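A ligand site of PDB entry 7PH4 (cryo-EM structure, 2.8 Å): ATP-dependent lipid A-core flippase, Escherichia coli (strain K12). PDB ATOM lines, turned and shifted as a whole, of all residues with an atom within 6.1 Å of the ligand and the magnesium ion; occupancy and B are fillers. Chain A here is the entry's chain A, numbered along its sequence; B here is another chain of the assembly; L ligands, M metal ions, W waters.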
ATOM      1  N   ASP A 128      11.394 -14.446   8.251  1.00  0.00           N
ATOM      2  CA  ASP A 128      11.550 -14.104   6.837  1.00  0.00           C
ATOM      3  C   ASP A 128      12.878 -13.412   6.575  1.00  0.00           C
ATOM      4  O   ASP A 128      13.549 -13.695   5.586  1.00  0.00           O
ATOM      5  CB  ASP A 128      10.401 -13.211   6.387  1.00  0.00           C
ATOM      6  CG  ASP A 128       9.097 -13.950   6.329  1.00  0.00           C
ATOM      7  OD1 ASP A 128       9.066 -15.134   6.742  1.00  0.00           O
ATOM      8  OD2 ASP A 128       8.097 -13.354   5.859  1.00  0.00           O
ATOM      9  N   TYR A 362       3.249  -5.751   3.556  1.00  0.00           N
ATOM     10  CA  TYR A 362       4.275  -6.590   4.136  1.00  0.00           C
ATOM     11  C   TYR A 362       5.397  -5.735   4.694  1.00  0.00           C
ATOM     12  O   TYR A 362       5.672  -4.656   4.187  1.00  0.00           O
ATOM     13  CB  TYR A 362       4.827  -7.559   3.109  1.00  0.00           C
ATOM     14  CG  TYR A 362       4.075  -8.860   3.029  1.00  0.00           C
ATOM     15  CD1 TYR A 362       4.218  -9.819   3.990  1.00  0.00           C
ATOM     16  CD2 TYR A 362       3.237  -9.127   1.979  1.00  0.00           C
ATOM     17  CE1 TYR A 362       3.552 -10.996   3.909  1.00  0.00           C
ATOM     18  CE2 TYR A 362       2.567 -10.296   1.902  1.00  0.00           C
ATOM     19  CZ  TYR A 362       2.724 -11.235   2.861  1.00  0.00           C
ATOM     20  OH  TYR A 362       2.051 -12.412   2.773  1.00  0.00           O
ATOM     21  N   PRO A 363       6.055  -6.177   5.762  1.00  0.00           N
ATOM     22  CA  PRO A 363       7.121  -5.372   6.356  1.00  0.00           C
ATOM     23  C   PRO A 363       8.200  -5.016   5.342  1.00  0.00           C
ATOM     24  O   PRO A 363       8.712  -5.861   4.615  1.00  0.00           O
ATOM     25  CB  PRO A 363       7.666  -6.274   7.466  1.00  0.00           C
ATOM     26  CG  PRO A 363       6.955  -7.571   7.326  1.00  0.00           C
ATOM     27  CD  PRO A 363       5.683  -7.291   6.645  1.00  0.00           C
ATOM     28  N   ARG A 365       8.002  -2.939   2.555  1.00  0.00           N
ATOM     29  CA  ARG A 365       7.564  -3.145   1.182  1.00  0.00           C
ATOM     30  C   ARG A 365       6.858  -1.966   0.552  1.00  0.00           C
ATOM     31  O   ARG A 365       6.789  -1.915  -0.683  1.00  0.00           O
ATOM     32  CB  ARG A 365       6.665  -4.380   1.108  1.00  0.00           C
ATOM     33  CG  ARG A 365       6.638  -5.068  -0.229  1.00  0.00           C
ATOM     34  CD  ARG A 365       7.984  -5.040  -0.884  1.00  0.00           C
ATOM     35  NE  ARG A 365       9.001  -5.786  -0.154  1.00  0.00           N
ATOM     36  CZ  ARG A 365       9.495  -6.963  -0.552  1.00  0.00           C
ATOM     37  NH1 ARG A 365      10.421  -7.577   0.164  1.00  0.00           N
ATOM     38  NH2 ARG A 365       9.055  -7.507  -1.686  1.00  0.00           N
ATOM     39  N   ALA A 369      -0.161  -5.221  -0.119  1.00  0.00           N
ATOM     40  CA  ALA A 369      -0.469  -6.514  -0.685  1.00  0.00           C
ATOM     41  C   ALA A 369      -1.971  -6.734  -0.792  1.00  0.00           C
ATOM     42  O   ALA A 369      -2.423  -7.431  -1.694  1.00  0.00           O
ATOM     43  CB  ALA A 369       0.163  -7.617   0.154  1.00  0.00           C
ATOM     44  N   GLY A 387      -7.657 -16.276  -8.596  1.00  0.00           N
ATOM     45  CA  GLY A 387      -7.008 -15.100  -9.134  1.00  0.00           C
ATOM     46  C   GLY A 387      -5.681 -15.486  -9.736  1.00  0.00           C
ATOM     47  O   GLY A 387      -5.245 -16.628  -9.658  1.00  0.00           O
ATOM     48  N   ARG A 388      -5.036 -14.507 -10.357  1.00  0.00           N
ATOM     49  CA  ARG A 388      -3.752 -14.777 -10.965  1.00  0.00           C
ATOM     50  C   ARG A 388      -2.689 -14.912  -9.890  1.00  0.00           C
ATOM     51  O   ARG A 388      -2.882 -14.546  -8.746  1.00  0.00           O
ATOM     52  CB  ARG A 388      -3.388 -13.686 -11.956  1.00  0.00           C
ATOM     53  CG  ARG A 388      -4.348 -13.603 -13.110  1.00  0.00           C
ATOM     54  CD  ARG A 388      -3.782 -12.776 -14.225  1.00  0.00           C
ATOM     55  NE  ARG A 388      -2.549 -13.354 -14.752  1.00  0.00           N
ATOM     56  CZ  ARG A 388      -1.966 -12.942 -15.867  1.00  0.00           C
ATOM     57  NH1 ARG A 388      -0.844 -13.518 -16.273  1.00  0.00           N
ATOM     58  NH2 ARG A 388      -2.492 -11.963 -16.574  1.00  0.00           N
ATOM     59  N   SER A 389      -1.556 -15.464 -10.281  1.00  0.00           N
ATOM     60  CA  SER A 389      -0.468 -15.677  -9.345  1.00  0.00           C
ATOM     61  C   SER A 389       0.144 -14.356  -8.921  1.00  0.00           C
ATOM     62  O   SER A 389       0.413 -13.479  -9.746  1.00  0.00           O
ATOM     63  CB  SER A 389       0.593 -16.574  -9.970  1.00  0.00           C
ATOM     64  OG  SER A 389       0.064 -17.859 -10.206  1.00  0.00           O
ATOM     65  N   GLY A 390       0.371 -14.213  -7.625  1.00  0.00           N
ATOM     66  CA  GLY A 390       0.880 -12.982  -7.065  1.00  0.00           C
ATOM     67  C   GLY A 390      -0.167 -11.963  -6.733  1.00  0.00           C
ATOM     68  O   GLY A 390       0.168 -10.788  -6.588  1.00  0.00           O
ATOM     69  N   SER A 391      -1.425 -12.368  -6.587  1.00  0.00           N
ATOM     70  CA  SER A 391      -2.508 -11.417  -6.402  1.00  0.00           C
ATOM     71  C   SER A 391      -2.956 -11.252  -4.949  1.00  0.00           C
ATOM     72  O   SER A 391      -3.654 -10.285  -4.652  1.00  0.00           O
ATOM     73  CB  SER A 391      -3.716 -11.822  -7.245  1.00  0.00           C
ATOM     74  OG  SER A 391      -4.046 -13.165  -7.011  1.00  0.00           O
ATOM     75  N   GLY A 392      -2.584 -12.153  -4.050  1.00  0.00           N
ATOM     76  CA  GLY A 392      -2.812 -11.914  -2.649  1.00  0.00           C
ATOM     77  C   GLY A 392      -3.747 -12.866  -1.951  1.00  0.00           C
ATOM     78  O   GLY A 392      -4.446 -12.476  -1.028  1.00  0.00           O
ATOM     79  N   LYS A 393      -3.788 -14.134  -2.381  1.00  0.00           N
ATOM     80  CA  LYS A 393      -4.629 -15.147  -1.779  1.00  0.00           C
ATOM     81  C   LYS A 393      -3.982 -15.797  -0.564  1.00  0.00           C
ATOM     82  O   LYS A 393      -4.586 -15.907   0.504  1.00  0.00           O
ATOM     83  CB  LYS A 393      -4.980 -16.191  -2.823  1.00  0.00           C
ATOM     84  CG  LYS A 393      -5.467 -15.611  -4.118  1.00  0.00           C
ATOM     85  CD  LYS A 393      -5.831 -16.682  -5.101  1.00  0.00           C
ATOM     86  CE  LYS A 393      -4.641 -17.478  -5.518  1.00  0.00           C
ATOM     87  NZ  LYS A 393      -3.790 -16.740  -6.448  1.00  0.00           N
ATOM     88  N   SER A 394      -2.741 -16.229  -0.712  1.00  0.00           N
ATOM     89  CA  SER A 394      -2.016 -16.744   0.423  1.00  0.00           C
ATOM     90  C   SER A 394      -1.829 -15.680   1.495  1.00  0.00           C
ATOM     91  O   SER A 394      -1.663 -16.017   2.661  1.00  0.00           O
ATOM     92  CB  SER A 394      -0.677 -17.305   0.001  1.00  0.00           C
ATOM     93  OG  SER A 394      -0.772 -17.996  -1.232  1.00  0.00           O
ATOM     94  N   THR A 395      -1.858 -14.400   1.125  1.00  0.00           N
ATOM     95  CA  THR A 395      -1.760 -13.343   2.116  1.00  0.00           C
ATOM     96  C   THR A 395      -3.026 -13.234   2.955  1.00  0.00           C
ATOM     97  O   THR A 395      -2.953 -13.018   4.162  1.00  0.00           O
ATOM     98  CB  THR A 395      -1.434 -12.025   1.445  1.00  0.00           C
ATOM     99  OG1 THR A 395      -0.126 -12.118   0.885  1.00  0.00           O
ATOM    100  CG2 THR A 395      -1.434 -10.900   2.419  1.00  0.00           C
ATOM    101  N   ILE A 396      -4.189 -13.366   2.337  1.00  0.00           N
ATOM    102  CA  ILE A 396      -5.428 -13.425   3.117  1.00  0.00           C
ATOM    103  C   ILE A 396      -5.403 -14.616   4.061  1.00  0.00           C
ATOM    104  O   ILE A 396      -5.730 -14.487   5.253  1.00  0.00           O
ATOM    105  CB  ILE A 396      -6.635 -13.486   2.171  1.00  0.00           C
ATOM    106  CG1 ILE A 396      -6.786 -12.167   1.426  1.00  0.00           C
ATOM    107  CG2 ILE A 396      -7.880 -13.821   2.920  1.00  0.00           C
ATOM    108  CD1 ILE A 396      -7.779 -12.208   0.305  1.00  0.00           C
ATOM    109  N   TYR A 404       0.793 -12.412  10.283  1.00  0.00           N
ATOM    110  CA  TYR A 404       1.097 -11.013  10.133  1.00  0.00           C
ATOM    111  C   TYR A 404      -0.092 -10.212  10.638  1.00  0.00           C
ATOM    112  O   TYR A 404      -1.224 -10.686  10.592  1.00  0.00           O
ATOM    113  CB  TYR A 404       1.348 -10.651   8.687  1.00  0.00           C
ATOM    114  CG  TYR A 404       2.519 -11.331   8.073  1.00  0.00           C
ATOM    115  CD1 TYR A 404       3.773 -10.791   8.172  1.00  0.00           C
ATOM    116  CD2 TYR A 404       2.377 -12.501   7.376  1.00  0.00           C
ATOM    117  CE1 TYR A 404       4.849 -11.400   7.612  1.00  0.00           C
ATOM    118  CE2 TYR A 404       3.442 -13.123   6.828  1.00  0.00           C
ATOM    119  CZ  TYR A 404       4.678 -12.565   6.945  1.00  0.00           C
ATOM    120  OH  TYR A 404       5.758 -13.183   6.381  1.00  0.00           O
ATOM    121  N   GLN A 435       0.614 -23.656   0.997  1.00  0.00           N
ATOM    122  CA  GLN A 435       1.042 -23.804  -0.391  1.00  0.00           C
ATOM    123  C   GLN A 435       2.362 -24.561  -0.480  1.00  0.00           C
ATOM    124  O   GLN A 435       2.535 -25.416  -1.355  1.00  0.00           O
ATOM    125  CB  GLN A 435       1.136 -22.444  -1.052  1.00  0.00           C
ATOM    126  CG  GLN A 435       2.224 -22.332  -2.070  1.00  0.00           C
ATOM    127  CD  GLN A 435       1.886 -21.382  -3.172  1.00  0.00           C
ATOM    128  OE1 GLN A 435       1.528 -20.235  -2.935  1.00  0.00           O
ATOM    129  NE2 GLN A 435       1.983 -21.861  -4.395  1.00  0.00           N
ATOM    130  N   ASP A 516      -4.774 -24.129   0.852  1.00  0.00           N
ATOM    131  CA  ASP A 516      -4.027 -23.175   0.048  1.00  0.00           C
ATOM    132  C   ASP A 516      -3.424 -23.905  -1.143  1.00  0.00           C
ATOM    133  O   ASP A 516      -2.244 -24.230  -1.173  1.00  0.00           O
ATOM    134  CB  ASP A 516      -2.968 -22.488   0.911  1.00  0.00           C
ATOM    135  CG  ASP A 516      -2.341 -21.301   0.233  1.00  0.00           C
ATOM    136  OD1 ASP A 516      -2.633 -21.074  -0.950  1.00  0.00           O
ATOM    137  OD2 ASP A 516      -1.572 -20.592   0.892  1.00  0.00           O
ATOM    138  N   GLU A 517      -4.260 -24.150  -2.138  1.00  0.00           N
ATOM    139  CA  GLU A 517      -3.906 -24.956  -3.303  1.00  0.00           C
ATOM    140  C   GLU A 517      -3.430 -26.334  -2.849  1.00  0.00           C
ATOM    141  O   GLU A 517      -2.280 -26.725  -3.049  1.00  0.00           O
ATOM    142  CB  GLU A 517      -2.868 -24.262  -4.167  1.00  0.00           C
ATOM    143  CG  GLU A 517      -3.322 -22.925  -4.641  1.00  0.00           C
ATOM    144  CD  GLU A 517      -2.472 -22.397  -5.746  1.00  0.00           C
ATOM    145  OE1 GLU A 517      -2.382 -21.154  -5.872  1.00  0.00           O
ATOM    146  OE2 GLU A 517      -1.882 -23.206  -6.486  1.00  0.00           O
ATOM    147  N   ILE A 546      -8.268 -21.947  -1.696  1.00  0.00           N
ATOM    148  CA  ILE A 546      -7.506 -21.116  -2.610  1.00  0.00           C
ATOM    149  C   ILE A 546      -7.117 -22.023  -3.761  1.00  0.00           C
ATOM    150  O   ILE A 546      -6.367 -22.982  -3.582  1.00  0.00           O
ATOM    151  CB  ILE A 546      -6.285 -20.507  -1.932  1.00  0.00           C
ATOM    152  CG1 ILE A 546      -6.728 -19.491  -0.881  1.00  0.00           C
ATOM    153  CG2 ILE A 546      -5.408 -19.859  -2.928  1.00  0.00           C
ATOM    154  CD1 ILE A 546      -5.743 -19.292   0.193  1.00  0.00           C
ATOM    155  N   HIS A 548      -6.300 -22.686  -8.141  1.00  0.00           N
ATOM    156  CA  HIS A 548      -6.037 -22.294  -9.513  1.00  0.00           C
ATOM    157  C   HIS A 548      -6.800 -23.118 -10.524  1.00  0.00           C
ATOM    158  O   HIS A 548      -7.082 -22.628 -11.622  1.00  0.00           O
ATOM    159  CB  HIS A 548      -4.537 -22.411  -9.821  1.00  0.00           C
ATOM    160  CG  HIS A 548      -3.759 -21.204  -9.435  1.00  0.00           C
ATOM    161  ND1 HIS A 548      -4.157 -19.927  -9.758  1.00  0.00           N
ATOM    162  CD2 HIS A 548      -2.593 -21.067  -8.777  1.00  0.00           C
ATOM    163  CE1 HIS A 548      -3.268 -19.059  -9.302  1.00  0.00           C
ATOM    164  NE2 HIS A 548      -2.313 -19.735  -8.703  1.00  0.00           N
ATOM    165  N   VAL B 490      11.051 -17.043   0.225  1.00  0.00           N
ATOM    166  CA  VAL B 490       9.870 -16.883   1.056  1.00  0.00           C
ATOM    167  C   VAL B 490       9.203 -15.530   0.858  1.00  0.00           C
ATOM    168  O   VAL B 490       8.015 -15.382   1.149  1.00  0.00           O
ATOM    169  CB  VAL B 490      10.242 -17.094   2.536  1.00  0.00           C
ATOM    170  CG1 VAL B 490      10.994 -15.910   3.056  1.00  0.00           C
ATOM    171  CG2 VAL B 490       9.008 -17.334   3.354  1.00  0.00           C
ATOM    172  N   LEU B 491       9.927 -14.532   0.356  1.00  0.00           N
ATOM    173  CA  LEU B 491       9.366 -13.223   0.090  1.00  0.00           C
ATOM    174  C   LEU B 491       8.701 -13.150  -1.266  1.00  0.00           C
ATOM    175  O   LEU B 491       8.565 -12.062  -1.815  1.00  0.00           O
ATOM    176  CB  LEU B 491      10.446 -12.152   0.187  1.00  0.00           C
ATOM    177  CG  LEU B 491      11.219 -12.153   1.493  1.00  0.00           C
ATOM    178  CD1 LEU B 491      12.239 -11.064   1.491  1.00  0.00           C
ATOM    179  CD2 LEU B 491      10.290 -12.002   2.657  1.00  0.00           C
ATOM    180  N   LEU B 492       8.297 -14.279  -1.815  1.00  0.00           N
ATOM    181  CA  LEU B 492       7.638 -14.361  -3.105  1.00  0.00           C
ATOM    182  C   LEU B 492       6.398 -15.210  -2.956  1.00  0.00           C
ATOM    183  O   LEU B 492       6.270 -16.001  -2.025  1.00  0.00           O
ATOM    184  CB  LEU B 492       8.552 -14.981  -4.155  1.00  0.00           C
ATOM    185  CG  LEU B 492       9.849 -14.318  -4.587  1.00  0.00           C
ATOM    186  CD1 LEU B 492      10.575 -15.235  -5.481  1.00  0.00           C
ATOM    187  CD2 LEU B 492       9.537 -13.060  -5.314  1.00  0.00           C
ATOM    188  N   SER B 493       5.472 -15.062  -3.885  1.00  0.00           N
ATOM    189  CA  SER B 493       4.359 -15.986  -3.914  1.00  0.00           C
ATOM    190  C   SER B 493       4.801 -17.283  -4.571  1.00  0.00           C
ATOM    191  O   SER B 493       5.873 -17.380  -5.155  1.00  0.00           O
ATOM    192  CB  SER B 493       3.169 -15.371  -4.623  1.00  0.00           C
ATOM    193  OG  SER B 493       3.399 -15.234  -5.996  1.00  0.00           O
ATOM    194  N   GLY B 494       3.963 -18.316  -4.461  1.00  0.00           N
ATOM    195  CA  GLY B 494       4.347 -19.624  -4.965  1.00  0.00           C
ATOM    196  C   GLY B 494       4.559 -19.655  -6.468  1.00  0.00           C
ATOM    197  O   GLY B 494       5.505 -20.269  -6.962  1.00  0.00           O
ATOM    198  N   GLY B 495       3.679 -19.003  -7.207  1.00  0.00           N
ATOM    199  CA  GLY B 495       3.865 -18.901  -8.634  1.00  0.00           C
ATOM    200  C   GLY B 495       5.089 -18.105  -9.013  1.00  0.00           C
ATOM    201  O   GLY B 495       5.725 -18.383 -10.026  1.00  0.00           O
ATOM    202  N   GLN B 496       5.445 -17.110  -8.209  1.00  0.00           N
ATOM    203  CA  GLN B 496       6.626 -16.315  -8.511  1.00  0.00           C
ATOM    204  C   GLN B 496       7.901 -17.107  -8.265  1.00  0.00           C
ATOM    205  O   GLN B 496       8.857 -16.996  -9.035  1.00  0.00           O
ATOM    206  CB  GLN B 496       6.585 -15.034  -7.712  1.00  0.00           C
ATOM    207  CG  GLN B 496       5.420 -14.177  -8.112  1.00  0.00           C
ATOM    208  CD  GLN B 496       5.285 -12.945  -7.294  1.00  0.00           C
ATOM    209  OE1 GLN B 496       5.913 -12.811  -6.257  1.00  0.00           O
ATOM    210  NE2 GLN B 496       4.457 -12.041  -7.740  1.00  0.00           N
ATOM    211  N   ARG B 499       8.191 -19.336 -11.274  1.00  0.00           N
ATOM    212  CA  ARG B 499       8.664 -18.675 -12.482  1.00  0.00           C
ATOM    213  C   ARG B 499      10.129 -18.291 -12.393  1.00  0.00           C
ATOM    214  O   ARG B 499      10.828 -18.277 -13.394  1.00  0.00           O
ATOM    215  CB  ARG B 499       7.811 -17.462 -12.778  1.00  0.00           C
ATOM    216  CG  ARG B 499       6.623 -17.814 -13.602  1.00  0.00           C
ATOM    217  CD  ARG B 499       5.736 -16.643 -13.754  1.00  0.00           C
ATOM    218  NE  ARG B 499       5.079 -16.332 -12.513  1.00  0.00           N
ATOM    219  CZ  ARG B 499       4.246 -15.323 -12.370  1.00  0.00           C
ATOM    220  NH1 ARG B 499       3.890 -14.926 -11.168  1.00  0.00           N
ATOM    221  NH2 ARG B 499       3.778 -14.710 -13.421  1.00  0.00           N
ATOM    222  N   ALA B 521       1.946 -24.154  -9.755  1.00  0.00           N
ATOM    223  CA  ALA B 521       1.474 -23.025  -8.977  1.00  0.00           C
ATOM    224  C   ALA B 521       1.041 -21.858  -9.846  1.00  0.00           C
ATOM    225  O   ALA B 521       0.732 -20.787  -9.315  1.00  0.00           O
ATOM    226  CB  ALA B 521       2.560 -22.553  -8.007  1.00  0.00           C
HETATM  227  P1  LIG L   1       0.212 -17.551  -6.050  1.00  0.00           P
HETATM  228  O1  LIG L   1       1.308 -17.542  -6.934  1.00  0.00           O
HETATM  229  O2  LIG L   1       0.574 -18.670  -5.225  1.00  0.00           O
HETATM  230  O3  LIG L   1      -0.989 -17.844  -6.760  1.00  0.00           O
HETATM  231  P2  LIG L   1      -0.886 -15.578  -4.153  1.00  0.00           P
HETATM  232  O4  LIG L   1      -1.933 -14.760  -4.738  1.00  0.00           O
HETATM  233  O5  LIG L   1      -1.254 -16.601  -3.178  1.00  0.00           O
HETATM  234  N1  LIG L   1       0.102 -16.167  -5.257  1.00  0.00           N
HETATM  235  P3  LIG L   1       0.652 -13.949  -2.156  1.00  0.00           P
HETATM  236  O6  LIG L   1      -0.353 -13.623  -1.145  1.00  0.00           O
HETATM  237  O7  LIG L   1       1.782 -14.784  -1.764  1.00  0.00           O
HETATM  238  O8  LIG L   1       0.027 -14.551  -3.471  1.00  0.00           O
HETATM  239  O9  LIG L   1       1.217 -12.645  -2.836  1.00  0.00           O
HETATM  240  C1  LIG L   1       0.821 -11.267  -2.650  1.00  0.00           C
HETATM  241  C2  LIG L   1       2.005 -10.375  -2.919  1.00  0.00           C
HETATM  242  O10 LIG L   1       2.842 -10.348  -1.744  1.00  0.00           O
HETATM  243  C3  LIG L   1       2.948 -10.814  -4.045  1.00  0.00           C
HETATM  244  O11 LIG L   1       3.597  -9.686  -4.564  1.00  0.00           O
HETATM  245  C4  LIG L   1       4.037 -11.577  -3.303  1.00  0.00           C
HETATM  246  O12 LIG L   1       5.254 -11.634  -4.004  1.00  0.00           O
HETATM  247  C5  LIG L   1       4.157 -10.739  -2.035  1.00  0.00           C
HETATM  248  N2  LIG L   1       4.595 -11.483  -0.910  1.00  0.00           N
HETATM  249  C6  LIG L   1       4.206 -12.709  -0.578  1.00  0.00           C
HETATM  250  N3  LIG L   1       4.744 -13.140   0.532  1.00  0.00           N
HETATM  251  C7  LIG L   1       5.542 -12.095   0.938  1.00  0.00           C
HETATM  252  C8  LIG L   1       6.377 -11.934   2.045  1.00  0.00           C
HETATM  253  N4  LIG L   1       6.485 -12.826   3.009  1.00  0.00           N
HETATM  254  N5  LIG L   1       7.035 -10.761   2.149  1.00  0.00           N
HETATM  255  C9  LIG L   1       6.891  -9.860   1.180  1.00  0.00           C
HETATM  256  N6  LIG L   1       6.127  -9.899   0.105  1.00  0.00           N
HETATM  257  C10 LIG L   1       5.472 -11.067   0.041  1.00  0.00           C
HETATM  258 MG    MG M   1      -0.199 -18.321  -3.358  1.00  0.00          MG
HETATM  259  O   HOH W   1      -1.967 -19.322  -3.378  1.00  0.00           O
HETATM  260  O   HOH W   2       1.368 -17.569  -2.298  1.00  0.00           O
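N of Gly 390 lies close to N1 of the ligand, at 3.1 Å.
Residues that only touch the ligand: Ser 389 (3.3 Å), Tyr 362 (3.5 Å), Val 490 of chain B (3.5 Å), Leu 491 of chain B (3.5 Å), Glu 517 (3.7 Å) and Leu 492 of chain B (3.7 Å).
Within 4 Å of the ligand: Asp 128, Tyr 362, Ser 389, Gly 390, Ser 391, Gly 392, Lys 393, Ser 394, Thr 395, Tyr 404, Gln 435, Glu 517, His 548, Val 490 of chain B, Leu 491 of chain B, Leu 492 of chain B, Ser 493 of chain B, Gly 494 of chain B, Gly 495 of chain B and Gln 496 of chain B.
The nearest printed residue that does not touch the ligand is Ala 521 of chain B (4.1 Å).
The backbone NH (N) of Gly 392 lies within hydrogen-bond range of an oxygen (O4) of the ligand (2.8 Å).
The side-chain hydroxyl of Ser 493 of chain B sits at hydrogen-bond distance from an oxygen (O1) of the ligand, at 3.3 Å.
An oxygen (O6) of the ligand sits at hydrogen-bond distance from the side-chain hydroxyl of Thr 395.
OE1 of Gln 496 of chain B lies within hydrogen-bond range of O12 of the ligand.
O2 of the ligand lies close to N of Gly 494 of chain B.
O3 of the ligand is in salt-bridge range of NZ of Lys 393 (3.0 Å).
The backbone NH (N) of Gly 495 of chain B lies within hydrogen-bond range of an oxygen (O1) of the ligand, at 2.8 Å.
The side-chain carboxylate (OD2) of Asp 128 lies within hydrogen-bond range of a nitrogen (N4) of the ligand, 3.3 Å away.
NE2 of His 548 is in hydrogen-bond range of O3 of the ligand (3.0 Å).
The backbone NH of Thr 395 sits at hydrogen-bond distance from an oxygen (O6) of the ligand (2.8 Å).
The side-chain amide oxygen of Gln 435 lies close to an oxygen (O2) of the ligand (2.9 Å).
N of Ser 394 lies close to O5 of the ligand, at 2.9 Å.
N of Ser 391 is in hydrogen-bond range of O4 of the ligand, at 3.1 Å.
N of Ser 493 of chain B lies within hydrogen-bond range of O12 of the ligand (3.4 Å).
O4 of the ligand lies within hydrogen-bond range of OG of Ser 391 (3.5 Å).
N4 of the ligand is in hydrogen-bond range of OH of Tyr 404 (3.5 Å).
O4 of the ligand is in hydrogen-bond range of N of Lys 393.
The magnesium ion is bound by an oxygen (O5) of the ligand (2.0 Å), water W1 (2.0 Å), water W2 (2.0 Å), an oxygen (O2) of the ligand (2.1 Å) and the side-chain hydroxyl of Ser 394 (2.2 Å).
The magnesium ion has five donor atoms within binding distance.
Slightly farther from the magnesium ion lies the side-chain amide oxygen (OE1) of Gln 435 (2.6 Å).
Water W1 bridges OD1 of Asp 516 (3.1 Å) and OE1 of Glu 517 (3.1 Å).
Water W2 lies within hydrogen-bond range of the side-chain amide oxygen (OE1) of Gln 435 (2.7 Å), an oxygen (O7) of the ligand (2.9 Å) and the backbone NH (N) of Gly 494 of chain B (3.5 Å).
Of the 30 residues printed, 2 come within 4 Å of the magnesium ion.
The backbone carbonyl oxygen (O) of Ala 521 of chain B is in hydrogen-bond range of a ring nitrogen (NE2) of His 548, 3.3 Å away.
The backbone NH (N) of Glu 517 sits at hydrogen-bond distance from the backbone carbonyl oxygen (O) of Ile 546 (2.8 Å).
OE1 of Gln 435 is in hydrogen-bond range of N of Gly 494 of chain B, at 3.5 Å.
NE2 of His 548 lies within hydrogen-bond range of OG of Ser 389, at 3.4 Å.
The backbone carbonyl oxygen of Arg 388 lies within hydrogen-bond range of the side-chain amino group of Lys 393 (3.3 Å).
The side-chain hydroxyl (OH) of Tyr 404 sits at hydrogen-bond distance from the side-chain carboxylate (OD2) of Asp 128 (2.4 Å).
A ring nitrogen (NE2) of His 548 sits close to the side-chain carboxylate (OE1) of Glu 517 (3.2 Å).
The side-chain hydroxyl of Ser 389 sits at hydrogen-bond distance from the backbone carbonyl oxygen of Ala 521 of chain B (3.1 Å).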
